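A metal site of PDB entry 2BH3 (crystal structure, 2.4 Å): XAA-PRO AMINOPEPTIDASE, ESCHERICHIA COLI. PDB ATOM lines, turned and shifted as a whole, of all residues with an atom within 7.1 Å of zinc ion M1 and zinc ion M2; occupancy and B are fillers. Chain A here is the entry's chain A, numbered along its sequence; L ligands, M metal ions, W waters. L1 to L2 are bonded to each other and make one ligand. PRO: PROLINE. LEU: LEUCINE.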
ATOM      1  N   TYR A 229     -21.510  -5.392  11.464  1.00  0.00           N
ATOM      2  CA  TYR A 229     -20.541  -4.686  10.634  1.00  0.00           C
ATOM      3  C   TYR A 229     -19.774  -5.723   9.830  1.00  0.00           C
ATOM      4  O   TYR A 229     -19.813  -6.903  10.143  1.00  0.00           O
ATOM      5  CB  TYR A 229     -19.580  -3.836  11.488  1.00  0.00           C
ATOM      6  CG  TYR A 229     -18.914  -4.612  12.606  1.00  0.00           C
ATOM      7  CD1 TYR A 229     -19.578  -4.849  13.800  1.00  0.00           C
ATOM      8  CD2 TYR A 229     -17.629  -5.131  12.461  1.00  0.00           C
ATOM      9  CE1 TYR A 229     -18.986  -5.568  14.822  1.00  0.00           C
ATOM     10  CE2 TYR A 229     -17.024  -5.861  13.490  1.00  0.00           C
ATOM     11  CZ  TYR A 229     -17.717  -6.064  14.666  1.00  0.00           C
ATOM     12  OH  TYR A 229     -17.169  -6.777  15.692  1.00  0.00           O
ATOM     13  N   ILE A 232     -13.886  -8.576  10.168  1.00  0.00           N
ATOM     14  CA  ILE A 232     -12.462  -8.351   9.997  1.00  0.00           C
ATOM     15  C   ILE A 232     -11.699  -9.597  10.409  1.00  0.00           C
ATOM     16  O   ILE A 232     -11.774 -10.032  11.555  1.00  0.00           O
ATOM     17  CB  ILE A 232     -12.006  -7.137  10.860  1.00  0.00           C
ATOM     18  CG1 ILE A 232     -12.634  -5.823  10.338  1.00  0.00           C
ATOM     19  CG2 ILE A 232     -10.458  -7.026  10.913  1.00  0.00           C
ATOM     20  CD1 ILE A 232     -12.935  -4.808  11.428  1.00  0.00           C
ATOM     21  N   ILE A 259      -9.388 -11.165  14.709  1.00  0.00           N
ATOM     22  CA  ILE A 259     -10.791 -11.248  14.280  1.00  0.00           C
ATOM     23  C   ILE A 259     -11.617 -10.229  15.030  1.00  0.00           C
ATOM     24  O   ILE A 259     -11.746 -10.324  16.234  1.00  0.00           O
ATOM     25  CB  ILE A 259     -11.379 -12.654  14.483  1.00  0.00           C
ATOM     26  CG1 ILE A 259     -10.474 -13.696  13.813  1.00  0.00           C
ATOM     27  CG2 ILE A 259     -12.812 -12.715  13.942  1.00  0.00           C
ATOM     28  CD1 ILE A 259     -11.054 -15.091  13.741  1.00  0.00           C
ATOM     29  N   ASP A 260     -12.138  -9.252  14.295  1.00  0.00           N
ATOM     30  CA  ASP A 260     -13.110  -8.293  14.799  1.00  0.00           C
ATOM     31  C   ASP A 260     -14.453  -8.587  14.108  1.00  0.00           C
ATOM     32  O   ASP A 260     -14.633  -8.336  12.911  1.00  0.00           O
ATOM     33  CB  ASP A 260     -12.635  -6.863  14.540  1.00  0.00           C
ATOM     34  CG  ASP A 260     -13.304  -5.825  15.457  1.00  0.00           C
ATOM     35  OD1 ASP A 260     -14.420  -6.059  15.964  1.00  0.00           O
ATOM     36  OD2 ASP A 260     -12.713  -4.763  15.664  1.00  0.00           O
ATOM     37  N   ALA A 261     -15.379  -9.124  14.890  1.00  0.00           N
ATOM     38  CA  ALA A 261     -16.653  -9.605  14.364  1.00  0.00           C
ATOM     39  C   ALA A 261     -17.765  -9.492  15.426  1.00  0.00           C
ATOM     40  O   ALA A 261     -17.531  -9.709  16.618  1.00  0.00           O
ATOM     41  CB  ALA A 261     -16.497 -11.034  13.881  1.00  0.00           C
ATOM     42  N   GLY A 262     -18.956  -9.148  14.957  1.00  0.00           N
ATOM     43  CA  GLY A 262     -20.120  -8.966  15.818  1.00  0.00           C
ATOM     44  C   GLY A 262     -21.410  -9.283  15.094  1.00  0.00           C
ATOM     45  O   GLY A 262     -21.566  -8.937  13.911  1.00  0.00           O
ATOM     46  N   GLY A 270     -23.395  -6.994  18.742  1.00  0.00           N
ATOM     47  CA  GLY A 270     -22.281  -7.544  19.475  1.00  0.00           C
ATOM     48  C   GLY A 270     -21.034  -7.011  18.795  1.00  0.00           C
ATOM     49  O   GLY A 270     -21.072  -6.609  17.632  1.00  0.00           O
ATOM     50  N   ASP A 271     -19.915  -6.975  19.511  1.00  0.00           N
ATOM     51  CA  ASP A 271     -18.678  -6.467  18.942  1.00  0.00           C
ATOM     52  C   ASP A 271     -17.462  -6.979  19.696  1.00  0.00           C
ATOM     53  O   ASP A 271     -17.065  -6.414  20.713  1.00  0.00           O
ATOM     54  CB  ASP A 271     -18.712  -4.930  18.921  1.00  0.00           C
ATOM     55  CG  ASP A 271     -17.474  -4.338  18.327  1.00  0.00           C
ATOM     56  OD1 ASP A 271     -16.639  -5.103  17.806  1.00  0.00           O
ATOM     57  OD2 ASP A 271     -17.320  -3.108  18.400  1.00  0.00           O
ATOM     58  N   ILE A 272     -16.865  -8.057  19.183  1.00  0.00           N
ATOM     59  CA  ILE A 272     -15.738  -8.689  19.853  1.00  0.00           C
ATOM     60  C   ILE A 272     -14.513  -8.725  18.931  1.00  0.00           C
ATOM     61  O   ILE A 272     -14.625  -8.916  17.703  1.00  0.00           O
ATOM     62  CB  ILE A 272     -16.082 -10.152  20.276  1.00  0.00           C
ATOM     63  CG1 ILE A 272     -17.142 -10.163  21.366  1.00  0.00           C
ATOM     64  CG2 ILE A 272     -14.826 -10.914  20.759  1.00  0.00           C
ATOM     65  CD1 ILE A 272     -17.491 -11.529  21.849  1.00  0.00           C
ATOM     66  N   THR A 273     -13.337  -8.531  19.536  1.00  0.00           N
ATOM     67  CA  THR A 273     -12.066  -8.824  18.856  1.00  0.00           C
ATOM     68  C   THR A 273     -11.295  -9.808  19.691  1.00  0.00           C
ATOM     69  O   THR A 273     -11.143  -9.642  20.907  1.00  0.00           O
ATOM     70  CB  THR A 273     -11.154  -7.586  18.639  1.00  0.00           C
ATOM     71  OG1 THR A 273     -11.918  -6.516  18.083  1.00  0.00           O
ATOM     72  CG2 THR A 273     -10.029  -7.936  17.660  1.00  0.00           C
ATOM     73  N   LEU A 352      -9.939   3.718  22.880  1.00  0.00           N
ATOM     74  CA  LEU A 352     -10.140   2.507  23.679  1.00  0.00           C
ATOM     75  C   LEU A 352     -11.569   1.978  23.630  1.00  0.00           C
ATOM     76  O   LEU A 352     -11.804   0.778  23.817  1.00  0.00           O
ATOM     77  CB  LEU A 352      -9.800   2.845  25.130  1.00  0.00           C
ATOM     78  CG  LEU A 352      -9.833   1.728  26.168  1.00  0.00           C
ATOM     79  CD1 LEU A 352      -8.845   0.641  25.790  1.00  0.00           C
ATOM     80  CD2 LEU A 352      -9.536   2.303  27.536  1.00  0.00           C
ATOM     81  N   SER A 353     -12.528   2.871  23.429  1.00  0.00           N
ATOM     82  CA  SER A 353     -13.925   2.548  23.675  1.00  0.00           C
ATOM     83  C   SER A 353     -14.874   3.346  22.777  1.00  0.00           C
ATOM     84  O   SER A 353     -14.671   4.532  22.549  1.00  0.00           O
ATOM     85  CB  SER A 353     -14.281   2.845  25.153  1.00  0.00           C
ATOM     86  OG  SER A 353     -13.550   2.032  26.063  1.00  0.00           O
ATOM     87  N   HIS A 354     -15.914   2.681  22.296  1.00  0.00           N
ATOM     88  CA  HIS A 354     -17.030   3.391  21.687  1.00  0.00           C
ATOM     89  C   HIS A 354     -18.330   2.898  22.297  1.00  0.00           C
ATOM     90  O   HIS A 354     -18.404   1.782  22.786  1.00  0.00           O
ATOM     91  CB  HIS A 354     -17.029   3.268  20.147  1.00  0.00           C
ATOM     92  CG  HIS A 354     -17.043   1.859  19.639  1.00  0.00           C
ATOM     93  ND1 HIS A 354     -18.198   1.097  19.600  1.00  0.00           N
ATOM     94  CD2 HIS A 354     -16.060   1.089  19.118  1.00  0.00           C
ATOM     95  CE1 HIS A 354     -17.896  -0.092  19.094  1.00  0.00           C
ATOM     96  NE2 HIS A 354     -16.620  -0.125  18.791  1.00  0.00           N
ATOM     97  N   TRP A 355     -19.363   3.746  22.251  1.00  0.00           N
ATOM     98  CA  TRP A 355     -20.702   3.326  22.639  1.00  0.00           C
ATOM     99  C   TRP A 355     -21.157   2.153  21.763  1.00  0.00           C
ATOM    100  O   TRP A 355     -20.782   2.063  20.592  1.00  0.00           O
ATOM    101  CB  TRP A 355     -21.715   4.464  22.472  1.00  0.00           C
ATOM    102  CG  TRP A 355     -21.395   5.798  23.114  1.00  0.00           C
ATOM    103  CD1 TRP A 355     -21.436   7.011  22.515  1.00  0.00           C
ATOM    104  CD2 TRP A 355     -20.999   6.025  24.477  1.00  0.00           C
ATOM    105  NE1 TRP A 355     -21.094   7.984  23.402  1.00  0.00           N
ATOM    106  CE2 TRP A 355     -20.805   7.412  24.617  1.00  0.00           C
ATOM    107  CE3 TRP A 355     -20.766   5.193  25.583  1.00  0.00           C
ATOM    108  CZ2 TRP A 355     -20.416   8.005  25.828  1.00  0.00           C
ATOM    109  CZ3 TRP A 355     -20.374   5.783  26.781  1.00  0.00           C
ATOM    110  CH2 TRP A 355     -20.211   7.183  26.895  1.00  0.00           C
ATOM    111  N   LEU A 356     -21.981   1.277  22.308  1.00  0.00           N
ATOM    112  CA  LEU A 356     -22.492   0.102  21.587  1.00  0.00           C
ATOM    113  C   LEU A 356     -24.015   0.007  21.755  1.00  0.00           C
ATOM    114  O   LEU A 356     -24.532   0.186  22.858  1.00  0.00           O
ATOM    115  CB  LEU A 356     -21.802  -1.171  22.119  1.00  0.00           C
ATOM    116  CG  LEU A 356     -22.141  -2.524  21.500  1.00  0.00           C
ATOM    117  CD1 LEU A 356     -21.644  -2.632  20.053  1.00  0.00           C
ATOM    118  CD2 LEU A 356     -21.557  -3.653  22.373  1.00  0.00           C
ATOM    119  N   VAL A 360     -23.153  -0.398  15.941  1.00  0.00           N
ATOM    120  CA  VAL A 360     -21.927  -0.909  16.561  1.00  0.00           C
ATOM    121  C   VAL A 360     -21.071   0.249  17.121  1.00  0.00           C
ATOM    122  O   VAL A 360     -20.617   0.172  18.264  1.00  0.00           O
ATOM    123  CB  VAL A 360     -21.155  -1.882  15.610  1.00  0.00           C
ATOM    124  CG1 VAL A 360     -20.557  -1.157  14.426  1.00  0.00           C
ATOM    125  CG2 VAL A 360     -20.085  -2.630  16.378  1.00  0.00           C
ATOM    126  N   HIS A 361     -20.886   1.312  16.349  1.00  0.00           N
ATOM    127  CA  HIS A 361     -20.417   2.606  16.850  1.00  0.00           C
ATOM    128  C   HIS A 361     -21.632   3.423  17.157  1.00  0.00           C
ATOM    129  O   HIS A 361     -22.169   4.128  16.273  1.00  0.00           O
ATOM    130  CB  HIS A 361     -19.576   3.352  15.825  1.00  0.00           C
ATOM    131  CG  HIS A 361     -18.346   2.616  15.413  1.00  0.00           C
ATOM    132  ND1 HIS A 361     -17.822   2.719  14.151  1.00  0.00           N
ATOM    133  CD2 HIS A 361     -17.580   1.739  16.079  1.00  0.00           C
ATOM    134  CE1 HIS A 361     -16.749   1.951  14.068  1.00  0.00           C
ATOM    135  NE2 HIS A 361     -16.587   1.341  15.219  1.00  0.00           N
ATOM    136  N   THR A 381     -17.561  -0.552  24.331  1.00  0.00           N
ATOM    137  CA  THR A 381     -16.502  -1.505  24.065  1.00  0.00           C
ATOM    138  C   THR A 381     -15.237  -1.115  24.815  1.00  0.00           C
ATOM    139  O   THR A 381     -15.073   0.027  25.258  1.00  0.00           O
ATOM    140  CB  THR A 381     -16.207  -1.615  22.569  1.00  0.00           C
ATOM    141  OG1 THR A 381     -15.600  -0.389  22.108  1.00  0.00           O
ATOM    142  CG2 THR A 381     -17.506  -1.916  21.808  1.00  0.00           C
ATOM    143  N   VAL A 382     -14.361  -2.102  24.978  1.00  0.00           N
ATOM    144  CA  VAL A 382     -13.050  -1.902  25.576  1.00  0.00           C
ATOM    145  C   VAL A 382     -12.121  -2.668  24.654  1.00  0.00           C
ATOM    146  O   VAL A 382     -12.146  -3.902  24.636  1.00  0.00           O
ATOM    147  CB  VAL A 382     -12.970  -2.427  27.038  1.00  0.00           C
ATOM    148  CG1 VAL A 382     -11.703  -1.927  27.708  1.00  0.00           C
ATOM    149  CG2 VAL A 382     -14.184  -1.999  27.843  1.00  0.00           C
ATOM    150  N   GLU A 383     -11.345  -1.936  23.867  1.00  0.00           N
ATOM    151  CA  GLU A 383     -10.577  -2.532  22.793  1.00  0.00           C
ATOM    152  C   GLU A 383      -9.196  -1.920  22.592  1.00  0.00           C
ATOM    153  O   GLU A 383      -8.923  -1.292  21.579  1.00  0.00           O
ATOM    154  CB  GLU A 383     -11.385  -2.488  21.484  1.00  0.00           C
ATOM    155  CG  GLU A 383     -11.852  -1.118  21.037  1.00  0.00           C
ATOM    156  CD  GLU A 383     -12.687  -1.197  19.789  1.00  0.00           C
ATOM    157  OE1 GLU A 383     -12.174  -1.691  18.751  1.00  0.00           O
ATOM    158  OE2 GLU A 383     -13.865  -0.783  19.848  1.00  0.00           O
ATOM    159  N   ARG A 404      -5.453  -6.854  18.765  1.00  0.00           N
ATOM    160  CA  ARG A 404      -6.523  -6.152  19.430  1.00  0.00           C
ATOM    161  C   ARG A 404      -7.325  -7.185  20.188  1.00  0.00           C
ATOM    162  O   ARG A 404      -7.557  -8.282  19.699  1.00  0.00           O
ATOM    163  CB  ARG A 404      -7.405  -5.384  18.428  1.00  0.00           C
ATOM    164  CG  ARG A 404      -8.624  -4.688  19.044  1.00  0.00           C
ATOM    165  CD  ARG A 404      -9.238  -3.615  18.121  1.00  0.00           C
ATOM    166  NE  ARG A 404      -9.866  -4.095  16.886  1.00  0.00           N
ATOM    167  CZ  ARG A 404      -9.326  -4.029  15.661  1.00  0.00           C
ATOM    168  NH1 ARG A 404      -8.108  -3.542  15.451  1.00  0.00           N
ATOM    169  NH2 ARG A 404     -10.002  -4.477  14.609  1.00  0.00           N
ATOM    170  N   GLU A 406     -10.928  -7.200  22.431  1.00  0.00           N
ATOM    171  CA  GLU A 406     -12.096  -6.371  22.677  1.00  0.00           C
ATOM    172  C   GLU A 406     -13.251  -7.106  23.334  1.00  0.00           C
ATOM    173  O   GLU A 406     -13.700  -8.143  22.851  1.00  0.00           O
ATOM    174  CB  GLU A 406     -12.574  -5.784  21.366  1.00  0.00           C
ATOM    175  CG  GLU A 406     -13.958  -5.168  21.435  1.00  0.00           C
ATOM    176  CD  GLU A 406     -14.302  -4.482  20.163  1.00  0.00           C
ATOM    177  OE1 GLU A 406     -13.805  -4.912  19.102  1.00  0.00           O
ATOM    178  OE2 GLU A 406     -15.090  -3.513  20.216  1.00  0.00           O
ATOM    179  N   ASP A 407     -13.734  -6.527  24.437  1.00  0.00           N
ATOM    180  CA  ASP A 407     -14.923  -6.978  25.136  1.00  0.00           C
ATOM    181  C   ASP A 407     -15.981  -5.859  25.093  1.00  0.00           C
ATOM    182  O   ASP A 407     -15.655  -4.689  24.846  1.00  0.00           O
ATOM    183  CB  ASP A 407     -14.601  -7.350  26.587  1.00  0.00           C
ATOM    184  CG  ASP A 407     -14.089  -8.792  26.741  1.00  0.00           C
ATOM    185  OD1 ASP A 407     -14.383  -9.654  25.877  1.00  0.00           O
ATOM    186  OD2 ASP A 407     -13.422  -9.077  27.770  1.00  0.00           O
ATOM    187  N   ASP A 408     -17.240  -6.245  25.308  1.00  0.00           N
ATOM    188  CA  ASP A 408     -18.386  -5.326  25.388  1.00  0.00           C
ATOM    189  C   ASP A 408     -18.907  -5.318  26.830  1.00  0.00           C
ATOM    190  O   ASP A 408     -19.110  -6.371  27.428  1.00  0.00           O
ATOM    191  CB  ASP A 408     -19.524  -5.767  24.457  1.00  0.00           C
ATOM    192  CG  ASP A 408     -19.082  -5.945  23.018  1.00  0.00           C
ATOM    193  OD1 ASP A 408     -18.153  -5.229  22.562  1.00  0.00           O
ATOM    194  OD2 ASP A 408     -19.680  -6.801  22.345  1.00  0.00           O
HETATM  195  N   PRO L   1     -12.862  -0.530  15.644  1.00  0.00           N
HETATM  196  CA  PRO L   1     -12.368   0.609  16.403  1.00  0.00           C
HETATM  197  C   PRO L   1     -12.982   1.957  15.988  1.00  0.00           C
HETATM  198  O   PRO L   1     -13.412   2.138  14.842  1.00  0.00           O
HETATM  199  CB  PRO L   1     -10.874   0.591  16.087  1.00  0.00           C
HETATM  200  CG  PRO L   1     -10.555  -0.821  15.805  1.00  0.00           C
HETATM  201  CD  PRO L   1     -11.763  -1.393  15.156  1.00  0.00           C
HETATM  202  N   LEU L   2     -13.033   2.872  16.941  1.00  0.00           N
HETATM  203  CA  LEU L   2     -13.393   4.272  16.700  1.00  0.00           C
HETATM  204  C   LEU L   2     -12.276   5.109  17.315  1.00  0.00           C
HETATM  205  O   LEU L   2     -11.808   6.094  16.764  1.00  0.00           O
HETATM  206  CB  LEU L   2     -14.756   4.621  17.319  1.00  0.00           C
HETATM  207  CG  LEU L   2     -15.318   6.029  17.080  1.00  0.00           C
HETATM  208  CD1 LEU L   2     -15.753   6.231  15.654  1.00  0.00           C
HETATM  209  CD2 LEU L   2     -16.478   6.302  18.021  1.00  0.00           C
HETATM  210  OXT LEU L   2     -11.819   4.786  18.412  1.00  0.00           O
HETATM  211 ZN    ZN M   1     -15.476  -1.927  18.782  1.00  0.00          ZN
HETATM  212 ZN    ZN M   2     -14.736  -4.454  17.227  1.00  0.00          ZN
HETATM  213 ZN    ZN M   3     -14.776   0.017  14.171  1.00  0.00          ZN
HETATM  214  O   HOH W   1     -14.348  -2.531  17.092  1.00  0.00           O
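Tyr 229 touches zinc ion M2 (OH to ZN, 3.7 Å). Thr 273 touches zinc ion M2 (OG1 to ZN, 3.6 Å). Five residues have an atom within 4 Å of zinc ion M2: Tyr 229, Asp 260, Asp 271, Thr 273 and Glu 406. The nearest printed residue that does not touch zinc ion M2 is Glu 383 (4.1 Å).
Zinc ion M1 is bound by water W1 (2.1 Å). NE2 of His 354 is bound to zinc ion M1, 2.1 Å away. The side-chain carboxylate (OE2) of Glu 406 is bound to zinc ion M1 (2.2 Å). The side-chain carboxylate (OD2) of Asp 271 binds zinc ion M1, 2.2 Å away. Zinc ion M1 is bound by OE2 of Glu 383. Zinc ion M1 has five donor atoms within binding distance.
CG2 of Thr 381 touches zinc ion M1, at 3.6 Å. Five residues have an atom within 4 Å of zinc ion M1: Asp 271, His 354, Thr 381, Glu 383 and Glu 406. The nearest printed residue that does not touch zinc ion M1 is His 361 (5.0 Å).
A nitrogen (N) of PRO L1 lies close to the side-chain carboxylate (OE1) of Glu 383, 3.4 Å away.
The side-chain carboxylate of Asp 260 sits close to the side-chain hydroxyl of Tyr 229 (2.9 Å). The side-chain carboxylate (OD2) of Asp 260 sits close to the guanidinium group (NH2) of Arg 404 (2.9 Å). OD2 of Asp 408 lies within hydrogen-bond range of N of Asp 271 (2.8 Å). The backbone NH (N) of Thr 381 is in hydrogen-bond range of the backbone carbonyl oxygen (O) of His 354, 2.9 Å away. The backbone carbonyl oxygen (O) of Thr 273 sits at hydrogen-bond distance from the backbone NH (N) of Glu 406 (2.9 Å). The guanidinium group (NE) of Arg 404 is in salt-bridge range of the side-chain carboxylate (OE1) of Glu 383. The side-chain hydroxyl (OG1) of Thr 273 lies within hydrogen-bond range of the guanidinium group (NE) of Arg 404 (3.4 Å). OH of Tyr 229 lies close to N of Ala 261 (3.1 Å).
Zinc ion M2 is bound by water W1 (2.0 Å), the side-chain carboxylate (OD1) of Asp 260 (2.1 Å), the side-chain carboxylate (OD1) of Asp 271 (2.1 Å), the side-chain carboxylate (OE1) of Glu 406 (2.1 Å) and the side-chain carboxylate (OD2) of Asp 260 (2.6 Å).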
